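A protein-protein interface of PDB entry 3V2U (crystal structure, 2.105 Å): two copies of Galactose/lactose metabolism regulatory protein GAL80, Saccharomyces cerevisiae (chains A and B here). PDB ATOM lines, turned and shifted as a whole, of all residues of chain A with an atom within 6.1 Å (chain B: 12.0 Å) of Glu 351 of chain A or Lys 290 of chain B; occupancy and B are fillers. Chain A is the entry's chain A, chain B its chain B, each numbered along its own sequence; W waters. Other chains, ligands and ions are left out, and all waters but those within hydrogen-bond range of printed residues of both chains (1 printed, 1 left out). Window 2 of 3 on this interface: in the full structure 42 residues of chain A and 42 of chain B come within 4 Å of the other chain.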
ATOM      1  N   HIS A 300       2.744  12.096 -11.794  1.00  0.00           N
ATOM      2  CA  HIS A 300       2.913  13.489 -11.372  1.00  0.00           C
ATOM      3  C   HIS A 300       4.378  13.911 -11.279  1.00  0.00           C
ATOM      4  O   HIS A 300       5.167  13.339 -10.514  1.00  0.00           O
ATOM      5  CB  HIS A 300       2.195  13.694 -10.030  1.00  0.00           C
ATOM      6  CG  HIS A 300       0.851  13.047 -10.000  1.00  0.00           C
ATOM      7  ND1 HIS A 300      -0.207  13.517 -10.750  1.00  0.00           N
ATOM      8  CD2 HIS A 300       0.415  11.913  -9.400  1.00  0.00           C
ATOM      9  CE1 HIS A 300      -1.245  12.712 -10.593  1.00  0.00           C
ATOM     10  NE2 HIS A 300      -0.893  11.734  -9.774  1.00  0.00           N
ATOM     11  N   LYS A 303       7.361  19.192 -13.201  1.00  0.00           N
ATOM     12  CA  LYS A 303       7.154  20.137 -14.298  1.00  0.00           C
ATOM     13  C   LYS A 303       5.939  19.833 -15.174  1.00  0.00           C
ATOM     14  O   LYS A 303       5.604  20.610 -16.043  1.00  0.00           O
ATOM     15  CB  LYS A 303       8.387  20.192 -15.193  1.00  0.00           C
ATOM     16  CG  LYS A 303       9.556  20.905 -14.569  1.00  0.00           C
ATOM     17  CD  LYS A 303      10.646  21.125 -15.615  1.00  0.00           C
ATOM     18  CE  LYS A 303      11.926  21.639 -14.982  1.00  0.00           C
ATOM     19  NZ  LYS A 303      13.058  21.655 -15.952  1.00  0.00           N
ATOM     20  N   GLY A 304       5.304  18.692 -14.964  1.00  0.00           N
ATOM     21  CA  GLY A 304       4.127  18.351 -15.738  1.00  0.00           C
ATOM     22  C   GLY A 304       3.544  17.056 -15.244  1.00  0.00           C
ATOM     23  O   GLY A 304       4.140  16.411 -14.386  1.00  0.00           O
ATOM     24  N   ASP A 305       2.389  16.678 -15.789  1.00  0.00           N
ATOM     25  CA  ASP A 305       1.737  15.430 -15.448  1.00  0.00           C
ATOM     26  C   ASP A 305       1.495  14.670 -16.714  1.00  0.00           C
ATOM     27  O   ASP A 305       1.332  15.248 -17.785  1.00  0.00           O
ATOM     28  CB  ASP A 305       0.349  15.672 -14.818  1.00  0.00           C
ATOM     29  CG  ASP A 305       0.390  15.826 -13.297  1.00  0.00           C
ATOM     30  OD1 ASP A 305       1.446  16.188 -12.741  1.00  0.00           O
ATOM     31  OD2 ASP A 305      -0.659  15.600 -12.650  1.00  0.00           O
ATOM     32  N   TYR A 324      -1.156  14.704 -21.587  1.00  0.00           N
ATOM     33  CA  TYR A 324       0.024  15.337 -21.032  1.00  0.00           C
ATOM     34  C   TYR A 324      -0.176  16.838 -20.898  1.00  0.00           C
ATOM     35  O   TYR A 324      -0.783  17.472 -21.760  1.00  0.00           O
ATOM     36  CB  TYR A 324       1.274  15.047 -21.886  1.00  0.00           C
ATOM     37  CG  TYR A 324       2.382  16.044 -21.592  1.00  0.00           C
ATOM     38  CD1 TYR A 324       3.184  15.912 -20.466  1.00  0.00           C
ATOM     39  CD2 TYR A 324       2.580  17.140 -22.405  1.00  0.00           C
ATOM     40  CE1 TYR A 324       4.176  16.836 -20.182  1.00  0.00           C
ATOM     41  CE2 TYR A 324       3.565  18.073 -22.133  1.00  0.00           C
ATOM     42  CZ  TYR A 324       4.361  17.917 -21.018  1.00  0.00           C
ATOM     43  OH  TYR A 324       5.334  18.853 -20.744  1.00  0.00           O
ATOM     44  N   SER A 325       0.339  17.396 -19.809  1.00  0.00           N
ATOM     45  CA  SER A 325       0.446  18.835 -19.686  1.00  0.00           C
ATOM     46  C   SER A 325       1.632  19.208 -18.801  1.00  0.00           C
ATOM     47  O   SER A 325       1.753  18.711 -17.668  1.00  0.00           O
ATOM     48  CB  SER A 325      -0.841  19.424 -19.100  1.00  0.00           C
ATOM     49  OG  SER A 325      -0.743  20.825 -19.090  1.00  0.00           O
ATOM     50  N   GLY A 326       2.497  20.074 -19.318  1.00  0.00           N
ATOM     51  CA  GLY A 326       3.626  20.589 -18.553  1.00  0.00           C
ATOM     52  C   GLY A 326       4.567  21.498 -19.342  1.00  0.00           C
ATOM     53  O   GLY A 326       4.148  22.160 -20.297  1.00  0.00           O
ATOM     54  N   THR A 327       5.844  21.519 -18.946  1.00  0.00           N
ATOM     55  CA  THR A 327       6.867  22.363 -19.590  1.00  0.00           C
ATOM     56  C   THR A 327       8.293  21.866 -19.326  1.00  0.00           C
ATOM     57  O   THR A 327       8.549  21.194 -18.327  1.00  0.00           O
ATOM     58  CB  THR A 327       6.778  23.831 -19.114  1.00  0.00           C
ATOM     59  OG1 THR A 327       7.773  24.617 -19.785  1.00  0.00           O
ATOM     60  CG2 THR A 327       7.008  23.927 -17.617  1.00  0.00           C
ATOM     61  N   ASP A 347       6.725  29.124 -26.338  1.00  0.00           N
ATOM     62  CA  ASP A 347       6.867  30.238 -25.407  1.00  0.00           C
ATOM     63  C   ASP A 347       7.254  29.690 -24.036  1.00  0.00           C
ATOM     64  O   ASP A 347       6.644  28.738 -23.544  1.00  0.00           O
ATOM     65  CB  ASP A 347       5.548  31.019 -25.333  1.00  0.00           C
ATOM     66  CG  ASP A 347       5.572  32.136 -24.297  1.00  0.00           C
ATOM     67  OD1 ASP A 347       6.131  31.939 -23.196  1.00  0.00           O
ATOM     68  OD2 ASP A 347       5.011  33.215 -24.585  1.00  0.00           O
ATOM     69  N   GLY A 349       6.941  30.662 -20.894  1.00  0.00           N
ATOM     70  CA  GLY A 349       6.052  30.711 -19.744  1.00  0.00           C
ATOM     71  C   GLY A 349       4.666  30.119 -19.932  1.00  0.00           C
ATOM     72  O   GLY A 349       3.717  30.537 -19.265  1.00  0.00           O
ATOM     73  N   LYS A 350       4.541  29.141 -20.824  1.00  0.00           N
ATOM     74  CA  LYS A 350       3.235  28.568 -21.135  1.00  0.00           C
ATOM     75  C   LYS A 350       3.263  27.043 -21.158  1.00  0.00           C
ATOM     76  O   LYS A 350       4.164  26.429 -21.735  1.00  0.00           O
ATOM     77  CB  LYS A 350       2.713  29.126 -22.463  1.00  0.00           C
ATOM     78  CG  LYS A 350       2.480  30.639 -22.436  1.00  0.00           C
ATOM     79  CD  LYS A 350       2.250  31.211 -23.833  1.00  0.00           C
ATOM     80  CE  LYS A 350       0.794  31.095 -24.276  1.00  0.00           C
ATOM     81  NZ  LYS A 350      -0.074  32.215 -23.789  1.00  0.00           N
ATOM     82  N   GLU A 351       2.275  26.432 -20.520  1.00  0.00           N
ATOM     83  CA  GLU A 351       2.175  24.976 -20.516  1.00  0.00           C
ATOM     84  C   GLU A 351       1.887  24.442 -21.911  1.00  0.00           C
ATOM     85  O   GLU A 351       1.164  25.056 -22.699  1.00  0.00           O
ATOM     86  CB  GLU A 351       1.100  24.506 -19.536  1.00  0.00           C
ATOM     87  CG  GLU A 351       1.403  24.841 -18.084  1.00  0.00           C
ATOM     88  CD  GLU A 351       1.543  23.606 -17.205  1.00  0.00           C
ATOM     89  OE1 GLU A 351       0.636  22.744 -17.226  1.00  0.00           O
ATOM     90  OE2 GLU A 351       2.562  23.498 -16.490  1.00  0.00           O
ATOM     91  N   ILE A 352       2.492  23.303 -22.217  1.00  0.00           N
ATOM     92  CA  ILE A 352       2.212  22.578 -23.432  1.00  0.00           C
ATOM     93  C   ILE A 352       1.156  21.522 -23.111  1.00  0.00           C
ATOM     94  O   ILE A 352       1.253  20.834 -22.106  1.00  0.00           O
ATOM     95  CB  ILE A 352       3.468  21.863 -23.920  1.00  0.00           C
ATOM     96  CG1 ILE A 352       4.534  22.882 -24.347  1.00  0.00           C
ATOM     97  CG2 ILE A 352       3.141  20.856 -25.030  1.00  0.00           C
ATOM     98  CD1 ILE A 352       5.915  22.251 -24.505  1.00  0.00           C
ATOM     99  N   MET A 353       0.154  21.404 -23.967  1.00  0.00           N
ATOM    100  CA  MET A 353      -0.882  20.392 -23.812  1.00  0.00           C
ATOM    101  C   MET A 353      -0.704  19.374 -24.944  1.00  0.00           C
ATOM    102  O   MET A 353      -0.502  19.748 -26.089  1.00  0.00           O
ATOM    103  CB  MET A 353      -2.258  21.052 -23.926  1.00  0.00           C
ATOM    104  CG  MET A 353      -3.420  20.054 -24.004  1.00  0.00           C
ATOM    105  SD  MET A 353      -3.948  19.479 -22.380  1.00  0.00           S
ATOM    106  CE  MET A 353      -4.257  17.743 -22.686  1.00  0.00           C
ATOM    107  N   ALA B 182      -7.321   9.591  -2.343  1.00  0.00           N
ATOM    108  CA  ALA B 182      -6.202  10.428  -2.752  1.00  0.00           C
ATOM    109  C   ALA B 182      -6.408  11.790  -2.105  1.00  0.00           C
ATOM    110  O   ALA B 182      -7.511  12.334  -2.138  1.00  0.00           O
ATOM    111  CB  ALA B 182      -6.140  10.532  -4.242  1.00  0.00           C
ATOM    112  N   GLY B 183      -5.364  12.303  -1.458  1.00  0.00           N
ATOM    113  CA  GLY B 183      -5.440  13.584  -0.776  1.00  0.00           C
ATOM    114  C   GLY B 183      -4.220  14.448  -1.024  1.00  0.00           C
ATOM    115  O   GLY B 183      -3.248  13.991  -1.618  1.00  0.00           O
ATOM    116  N   ASN B 184      -4.276  15.708  -0.596  1.00  0.00           N
ATOM    117  CA  ASN B 184      -3.148  16.618  -0.740  1.00  0.00           C
ATOM    118  C   ASN B 184      -2.956  17.387   0.555  1.00  0.00           C
ATOM    119  O   ASN B 184      -3.929  17.874   1.136  1.00  0.00           O
ATOM    120  CB  ASN B 184      -3.371  17.589  -1.905  1.00  0.00           C
ATOM    121  CG  ASN B 184      -2.110  18.375  -2.266  1.00  0.00           C
ATOM    122  OD1 ASN B 184      -1.692  19.257  -1.523  1.00  0.00           O
ATOM    123  ND2 ASN B 184      -1.508  18.069  -3.427  1.00  0.00           N
ATOM    124  N   TYR B 190       7.364  21.482  -3.183  1.00  0.00           N
ATOM    125  CA  TYR B 190       8.740  21.936  -3.413  1.00  0.00           C
ATOM    126  C   TYR B 190       9.041  23.376  -2.991  1.00  0.00           C
ATOM    127  O   TYR B 190      10.212  23.747  -2.820  1.00  0.00           O
ATOM    128  CB  TYR B 190       9.099  21.758  -4.897  1.00  0.00           C
ATOM    129  CG  TYR B 190       9.082  20.308  -5.301  1.00  0.00           C
ATOM    130  CD1 TYR B 190       7.939  19.733  -5.834  1.00  0.00           C
ATOM    131  CD2 TYR B 190      10.199  19.498  -5.098  1.00  0.00           C
ATOM    132  CE1 TYR B 190       7.909  18.396  -6.188  1.00  0.00           C
ATOM    133  CE2 TYR B 190      10.185  18.156  -5.443  1.00  0.00           C
ATOM    134  CZ  TYR B 190       9.032  17.614  -5.985  1.00  0.00           C
ATOM    135  OH  TYR B 190       9.013  16.295  -6.330  1.00  0.00           O
ATOM    136  N   GLU B 191       7.994  24.178  -2.820  1.00  0.00           N
ATOM    137  CA  GLU B 191       8.141  25.599  -2.502  1.00  0.00           C
ATOM    138  C   GLU B 191       7.414  25.928  -1.206  1.00  0.00           C
ATOM    139  O   GLU B 191       6.439  25.267  -0.859  1.00  0.00           O
ATOM    140  CB  GLU B 191       7.572  26.453  -3.652  1.00  0.00           C
ATOM    141  CG  GLU B 191       8.157  26.089  -5.009  1.00  0.00           C
ATOM    142  CD  GLU B 191       7.575  26.882  -6.166  1.00  0.00           C
ATOM    143  OE1 GLU B 191       6.385  27.249  -6.108  1.00  0.00           O
ATOM    144  OE2 GLU B 191       8.314  27.134  -7.145  1.00  0.00           O
ATOM    145  N   ARG B 252      10.407  32.043  -7.140  1.00  0.00           N
ATOM    146  CA  ARG B 252      11.439  31.533  -6.235  1.00  0.00           C
ATOM    147  C   ARG B 252      12.425  32.640  -5.891  1.00  0.00           C
ATOM    148  O   ARG B 252      12.814  33.420  -6.752  1.00  0.00           O
ATOM    149  CB  ARG B 252      12.152  30.316  -6.832  1.00  0.00           C
ATOM    150  CG  ARG B 252      11.245  29.092  -6.922  1.00  0.00           C
ATOM    151  CD  ARG B 252      11.957  27.821  -7.389  1.00  0.00           C
ATOM    152  NE  ARG B 252      10.980  26.733  -7.494  1.00  0.00           N
ATOM    153  CZ  ARG B 252      11.279  25.443  -7.643  1.00  0.00           C
ATOM    154  NH1 ARG B 252      12.538  25.048  -7.702  1.00  0.00           N
ATOM    155  NH2 ARG B 252      10.310  24.542  -7.727  1.00  0.00           N
ATOM    156  N   LYS B 283      -0.349  13.224  -1.381  1.00  0.00           N
ATOM    157  CA  LYS B 283       0.681  14.076  -1.925  1.00  0.00           C
ATOM    158  C   LYS B 283       0.936  15.247  -0.965  1.00  0.00           C
ATOM    159  O   LYS B 283      -0.011  15.832  -0.439  1.00  0.00           O
ATOM    160  CB  LYS B 283       0.191  14.585  -3.295  1.00  0.00           C
ATOM    161  CG  LYS B 283       1.274  15.101  -4.229  1.00  0.00           C
ATOM    162  CD  LYS B 283       0.695  15.549  -5.598  1.00  0.00           C
ATOM    163  CE  LYS B 283       1.786  15.715  -6.676  1.00  0.00           C
ATOM    164  NZ  LYS B 283       2.557  17.015  -6.543  1.00  0.00           N
ATOM    165  N   GLY B 285       1.987  18.409  -1.325  1.00  0.00           N
ATOM    166  CA  GLY B 285       1.589  19.752  -1.709  1.00  0.00           C
ATOM    167  C   GLY B 285       1.581  19.948  -3.210  1.00  0.00           C
ATOM    168  O   GLY B 285       1.258  19.031  -3.968  1.00  0.00           O
ATOM    169  N   LYS B 286       1.923  21.156  -3.638  1.00  0.00           N
ATOM    170  CA  LYS B 286       2.031  21.490  -5.058  1.00  0.00           C
ATOM    171  C   LYS B 286       3.271  20.849  -5.706  1.00  0.00           C
ATOM    172  O   LYS B 286       4.235  20.528  -5.015  1.00  0.00           O
ATOM    173  CB  LYS B 286       2.057  23.009  -5.220  1.00  0.00           C
ATOM    174  CG  LYS B 286       0.752  23.674  -4.718  1.00  0.00           C
ATOM    175  CD  LYS B 286       0.721  25.150  -5.050  1.00  0.00           C
ATOM    176  CE  LYS B 286      -0.571  25.792  -4.586  1.00  0.00           C
ATOM    177  NZ  LYS B 286      -0.705  25.753  -3.100  1.00  0.00           N
ATOM    178  N   PRO B 287       3.249  20.670  -7.037  1.00  0.00           N
ATOM    179  CA  PRO B 287       2.139  21.050  -7.926  1.00  0.00           C
ATOM    180  C   PRO B 287       0.910  20.181  -7.699  1.00  0.00           C
ATOM    181  O   PRO B 287       1.042  19.017  -7.336  1.00  0.00           O
ATOM    182  CB  PRO B 287       2.708  20.791  -9.336  1.00  0.00           C
ATOM    183  CG  PRO B 287       4.210  20.775  -9.156  1.00  0.00           C
ATOM    184  CD  PRO B 287       4.421  20.186  -7.792  1.00  0.00           C
ATOM    185  N   THR B 288      -0.278  20.739  -7.899  1.00  0.00           N
ATOM    186  CA  THR B 288      -1.483  19.939  -7.801  1.00  0.00           C
ATOM    187  C   THR B 288      -1.596  19.065  -9.057  1.00  0.00           C
ATOM    188  O   THR B 288      -0.931  19.315 -10.068  1.00  0.00           O
ATOM    189  CB  THR B 288      -2.712  20.830  -7.719  1.00  0.00           C
ATOM    190  OG1 THR B 288      -2.664  21.765  -8.797  1.00  0.00           O
ATOM    191  CG2 THR B 288      -2.734  21.589  -6.385  1.00  0.00           C
ATOM    192  N   LYS B 289      -2.458  18.070  -9.005  1.00  0.00           N
ATOM    193  CA  LYS B 289      -2.593  17.157 -10.132  1.00  0.00           C
ATOM    194  C   LYS B 289      -3.293  17.852 -11.280  1.00  0.00           C
ATOM    195  O   LYS B 289      -4.141  18.711 -11.072  1.00  0.00           O
ATOM    196  CB  LYS B 289      -3.340  15.907  -9.710  1.00  0.00           C
ATOM    197  CG  LYS B 289      -2.593  15.126  -8.632  1.00  0.00           C
ATOM    198  CD  LYS B 289      -3.415  13.941  -8.163  1.00  0.00           C
ATOM    199  CE  LYS B 289      -2.760  13.286  -6.962  1.00  0.00           C
ATOM    200  NZ  LYS B 289      -3.420  12.001  -6.629  1.00  0.00           N
ATOM    201  N   LYS B 290      -2.915  17.511 -12.501  1.00  0.00           N
ATOM    202  CA  LYS B 290      -3.476  18.222 -13.640  1.00  0.00           C
ATOM    203  C   LYS B 290      -4.744  17.588 -14.207  1.00  0.00           C
ATOM    204  O   LYS B 290      -5.554  18.282 -14.815  1.00  0.00           O
ATOM    205  CB  LYS B 290      -2.428  18.391 -14.737  1.00  0.00           C
ATOM    206  CG  LYS B 290      -1.375  19.434 -14.392  1.00  0.00           C
ATOM    207  CD  LYS B 290      -0.395  19.626 -15.521  1.00  0.00           C
ATOM    208  CE  LYS B 290       0.904  20.210 -14.999  1.00  0.00           C
ATOM    209  NZ  LYS B 290       0.666  21.504 -14.304  1.00  0.00           N
ATOM    210  N   PHE B 291      -4.924  16.287 -14.017  1.00  0.00           N
ATOM    211  CA  PHE B 291      -5.972  15.590 -14.753  1.00  0.00           C
ATOM    212  C   PHE B 291      -6.943  14.877 -13.833  1.00  0.00           C
ATOM    213  O   PHE B 291      -7.838  14.160 -14.284  1.00  0.00           O
ATOM    214  CB  PHE B 291      -5.355  14.600 -15.748  1.00  0.00           C
ATOM    215  CG  PHE B 291      -4.579  15.260 -16.839  1.00  0.00           C
ATOM    216  CD1 PHE B 291      -5.214  16.107 -17.743  1.00  0.00           C
ATOM    217  CD2 PHE B 291      -3.216  15.033 -16.978  1.00  0.00           C
ATOM    218  CE1 PHE B 291      -4.486  16.746 -18.755  1.00  0.00           C
ATOM    219  CE2 PHE B 291      -2.482  15.652 -17.983  1.00  0.00           C
ATOM    220  CZ  PHE B 291      -3.111  16.507 -18.877  1.00  0.00           C
ATOM    221  N   THR B 292      -6.775  15.112 -12.540  1.00  0.00           N
ATOM    222  CA  THR B 292      -7.516  14.411 -11.507  1.00  0.00           C
ATOM    223  C   THR B 292      -7.759  15.399 -10.372  1.00  0.00           C
ATOM    224  O   THR B 292      -6.914  16.257 -10.124  1.00  0.00           O
ATOM    225  CB  THR B 292      -6.651  13.231 -10.978  1.00  0.00           C
ATOM    226  OG1 THR B 292      -6.015  12.582 -12.094  1.00  0.00           O
ATOM    227  CG2 THR B 292      -7.492  12.218 -10.234  1.00  0.00           C
ATOM    228  N   LYS B 293      -8.905  15.295  -9.698  1.00  0.00           N
ATOM    229  CA  LYS B 293      -9.185  16.115  -8.507  1.00  0.00           C
ATOM    230  C   LYS B 293      -8.159  15.804  -7.416  1.00  0.00           C
ATOM    231  O   LYS B 293      -7.672  14.675  -7.319  1.00  0.00           O
ATOM    232  CB  LYS B 293     -10.592  15.834  -7.975  1.00  0.00           C
ATOM    233  CG  LYS B 293     -11.706  16.288  -8.876  1.00  0.00           C
ATOM    234  CD  LYS B 293     -11.754  17.791  -8.920  1.00  0.00           C
ATOM    235  CE  LYS B 293     -13.016  18.281  -9.655  1.00  0.00           C
ATOM    236  NZ  LYS B 293     -12.854  18.286 -11.124  1.00  0.00           N
ATOM    237  N   ASN B 294      -7.838  16.792  -6.590  1.00  0.00           N
ATOM    238  CA  ASN B 294      -6.786  16.618  -5.586  1.00  0.00           C
ATOM    239  C   ASN B 294      -7.246  15.935  -4.306  1.00  0.00           C
ATOM    240  O   ASN B 294      -6.435  15.455  -3.508  1.00  0.00           O
ATOM    241  CB  ASN B 294      -6.109  17.952  -5.288  1.00  0.00           C
ATOM    242  CG  ASN B 294      -5.369  18.477  -6.474  1.00  0.00           C
ATOM    243  OD1 ASN B 294      -4.317  17.954  -6.833  1.00  0.00           O
ATOM    244  ND2 ASN B 294      -5.922  19.494  -7.118  1.00  0.00           N
ATOM    245  N   LEU B 295      -8.553  15.908  -4.118  1.00  0.00           N
ATOM    246  CA  LEU B 295      -9.146  15.150  -3.027  1.00  0.00           C
ATOM    247  C   LEU B 295     -10.204  14.232  -3.603  1.00  0.00           C
ATOM    248  O   LEU B 295     -11.149  14.682  -4.244  1.00  0.00           O
ATOM    249  CB  LEU B 295      -9.772  16.074  -1.978  1.00  0.00           C
ATOM    250  CG  LEU B 295     -10.496  15.302  -0.865  1.00  0.00           C
ATOM    251  CD1 LEU B 295      -9.519  14.392  -0.125  1.00  0.00           C
ATOM    252  CD2 LEU B 295     -11.201  16.243   0.103  1.00  0.00           C
ATOM    253  N   VAL B 296     -10.033  12.934  -3.391  1.00  0.00           N
ATOM    254  CA  VAL B 296     -10.976  11.949  -3.924  1.00  0.00           C
ATOM    255  C   VAL B 296     -11.162  10.846  -2.906  1.00  0.00           C
ATOM    256  O   VAL B 296     -10.189  10.345  -2.356  1.00  0.00           O
ATOM    257  CB  VAL B 296     -10.472  11.305  -5.240  1.00  0.00           C
ATOM    258  CG1 VAL B 296     -11.369  10.126  -5.638  1.00  0.00           C
ATOM    259  CG2 VAL B 296     -10.395  12.343  -6.362  1.00  0.00           C
ATOM    260  N   GLU B 309     -15.544  14.140  -4.213  1.00  0.00           N
ATOM    261  CA  GLU B 309     -14.421  14.883  -4.778  1.00  0.00           C
ATOM    262  C   GLU B 309     -14.393  16.302  -4.259  1.00  0.00           C
ATOM    263  O   GLU B 309     -15.430  16.925  -4.069  1.00  0.00           O
ATOM    264  CB  GLU B 309     -14.500  14.946  -6.311  1.00  0.00           C
ATOM    265  CG  GLU B 309     -14.469  13.621  -7.012  1.00  0.00           C
ATOM    266  CD  GLU B 309     -14.301  13.760  -8.522  1.00  0.00           C
ATOM    267  OE1 GLU B 309     -14.877  14.696  -9.129  1.00  0.00           O
ATOM    268  OE2 GLU B 309     -13.584  12.925  -9.103  1.00  0.00           O
ATOM    269  N   GLY B 310     -13.196  16.837  -4.091  1.00  0.00           N
ATOM    270  CA  GLY B 310     -13.048  18.230  -3.716  1.00  0.00           C
ATOM    271  C   GLY B 310     -11.941  18.887  -4.515  1.00  0.00           C
ATOM    272  O   GLY B 310     -10.862  18.313  -4.666  1.00  0.00           O
ATOM    273  N   ASP B 311     -12.219  20.069  -5.048  1.00  0.00           N
ATOM    274  CA  ASP B 311     -11.230  20.808  -5.820  1.00  0.00           C
ATOM    275  C   ASP B 311     -10.469  21.758  -4.913  1.00  0.00           C
ATOM    276  O   ASP B 311      -9.336  22.130  -5.202  1.00  0.00           O
ATOM    277  CB  ASP B 311     -11.897  21.595  -6.950  1.00  0.00           C
ATOM    278  CG  ASP B 311     -13.404  21.443  -6.958  1.00  0.00           C
ATOM    279  OD1 ASP B 311     -13.901  20.385  -6.521  1.00  0.00           O
ATOM    280  OD2 ASP B 311     -14.092  22.381  -7.412  1.00  0.00           O
HETATM  281  O   HOH W   1      -2.993  14.245 -13.017  1.00  0.00           O
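The side-chain carboxylate (OD2) of Asp 305 of chain A sits at hydrogen-bond distance from the backbone NH (N) of Lys 290 of chain B, 3.0 Å away. The side-chain carboxylate of Glu 351 of chain A lies within salt-bridge range of the side-chain amino group of Lys 290 of chain B.
The side-chain carboxylate of Asp 305 of chain A is in hydrogen-bond range of a ring nitrogen (ND1) of His 300 of chain A (2.9 Å). The backbone carbonyl oxygen (O) of Ser 325 of chain A lies within hydrogen-bond range of the backbone NH (N) of Asp 305 of chain A (2.8 Å). N of Gly 326 of chain A sits close to OH of Tyr 324 of chain A (3.4 Å). OG of Ser 325 of chain A sits at hydrogen-bond distance from OE1 of Glu 351 of chain A. The backbone carbonyl oxygen (O) of Gly 183 of chain B sits at hydrogen-bond distance from the backbone NH (N) of Lys 283 of chain B. NZ of Lys 283 of chain B sits at hydrogen-bond distance from O of Pro 287 of chain B (2.6 Å).
His 300 of chain A touches Lys 283 of chain B (CB to CE, 3.9 Å). CE1 of His 300 of chain A touches CG of Lys 289 of chain B, at 3.4 Å. Lys 290 of chain B touches Gly 304 of chain A. Asp 305 of chain A touches Lys 289 of chain B. Asp 305 of chain A touches Phe 291 of chain B. CZ of Phe 291 of chain B touches C of Tyr 324 of chain A, 3.6 Å away. Ser 325 of chain A touches Lys 290 of chain B (O to CD, 3.2 Å). N of Ser 325 of chain A touches CZ of Phe 291 of chain B, at 3.7 Å.
Glu 351 of chain A touches one residue of chain B. Printed residues of chain A within 4 Å of Lys 290 of chain B: Gly 304 (3.8 Å), Asp 305 (3.0 Å), Ser 325 (3.2 Å) and Glu 351 (3.2 Å). Gly 304 of chain A touches one residue of chain B. Of the printed residues of chain B, Asp 305 of chain A touches Lys 289 (3.5 Å), Lys 290 (3.0 Å) and Phe 291 (3.8 Å). Of chain B, only Lys 290 and Phe 291 come within 4 Å of Ser 325 of chain A. Gly 326 of chain A touches none of the printed residues of chain B. No residue of chain B comes within 4 Å of Thr 327 of chain A. No residue of chain B comes within 4 Å of Gly 349 of chain A. No residue of chain B comes within 4 Å of Ile 352 of chain A. Printed residues of chain A within 4 Å of Lys 289 of chain B: His 300 and Asp 305. Of the printed residues of chain B, Tyr 324 of chain A touches Phe 291. Printed residues of chain A within 4 Å of Lys 283 of chain B: His 300 (3.9 Å). The nearest residue of chain B that does not touch Glu 351 of chain A is Phe 291 of chain B (7.5 Å).
Of the 22 printed residues of chain B, 4 touch a printed residue of chain A. Printed residues of chain B that touch a printed residue of chain A: Lys 283, Lys 289, Lys 290 and Phe 291. Hydrophobic or aromatic side chains of chain B within 4 Å of the printed part of chain A: Phe 291. Along chain B the printed residues that touch a printed residue of chain A span positions 283 to 291. Among the printed residues, Asp or Glu carboxylates within 4 Å of a Lys or Arg side-chain nitrogen of the other chain: Glu 351 of chain A with Lys 290 of chain B.
No position is printed for both chains. Of the 10 pairs that touch across the chains among the printed residues, none has its exchanged pair printed and touching as well.
Water W1 lies within hydrogen-bond range of OD2 of Asp 305 of chain A, N of Phe 291 of chain B and N of Lys 290 of chain B.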
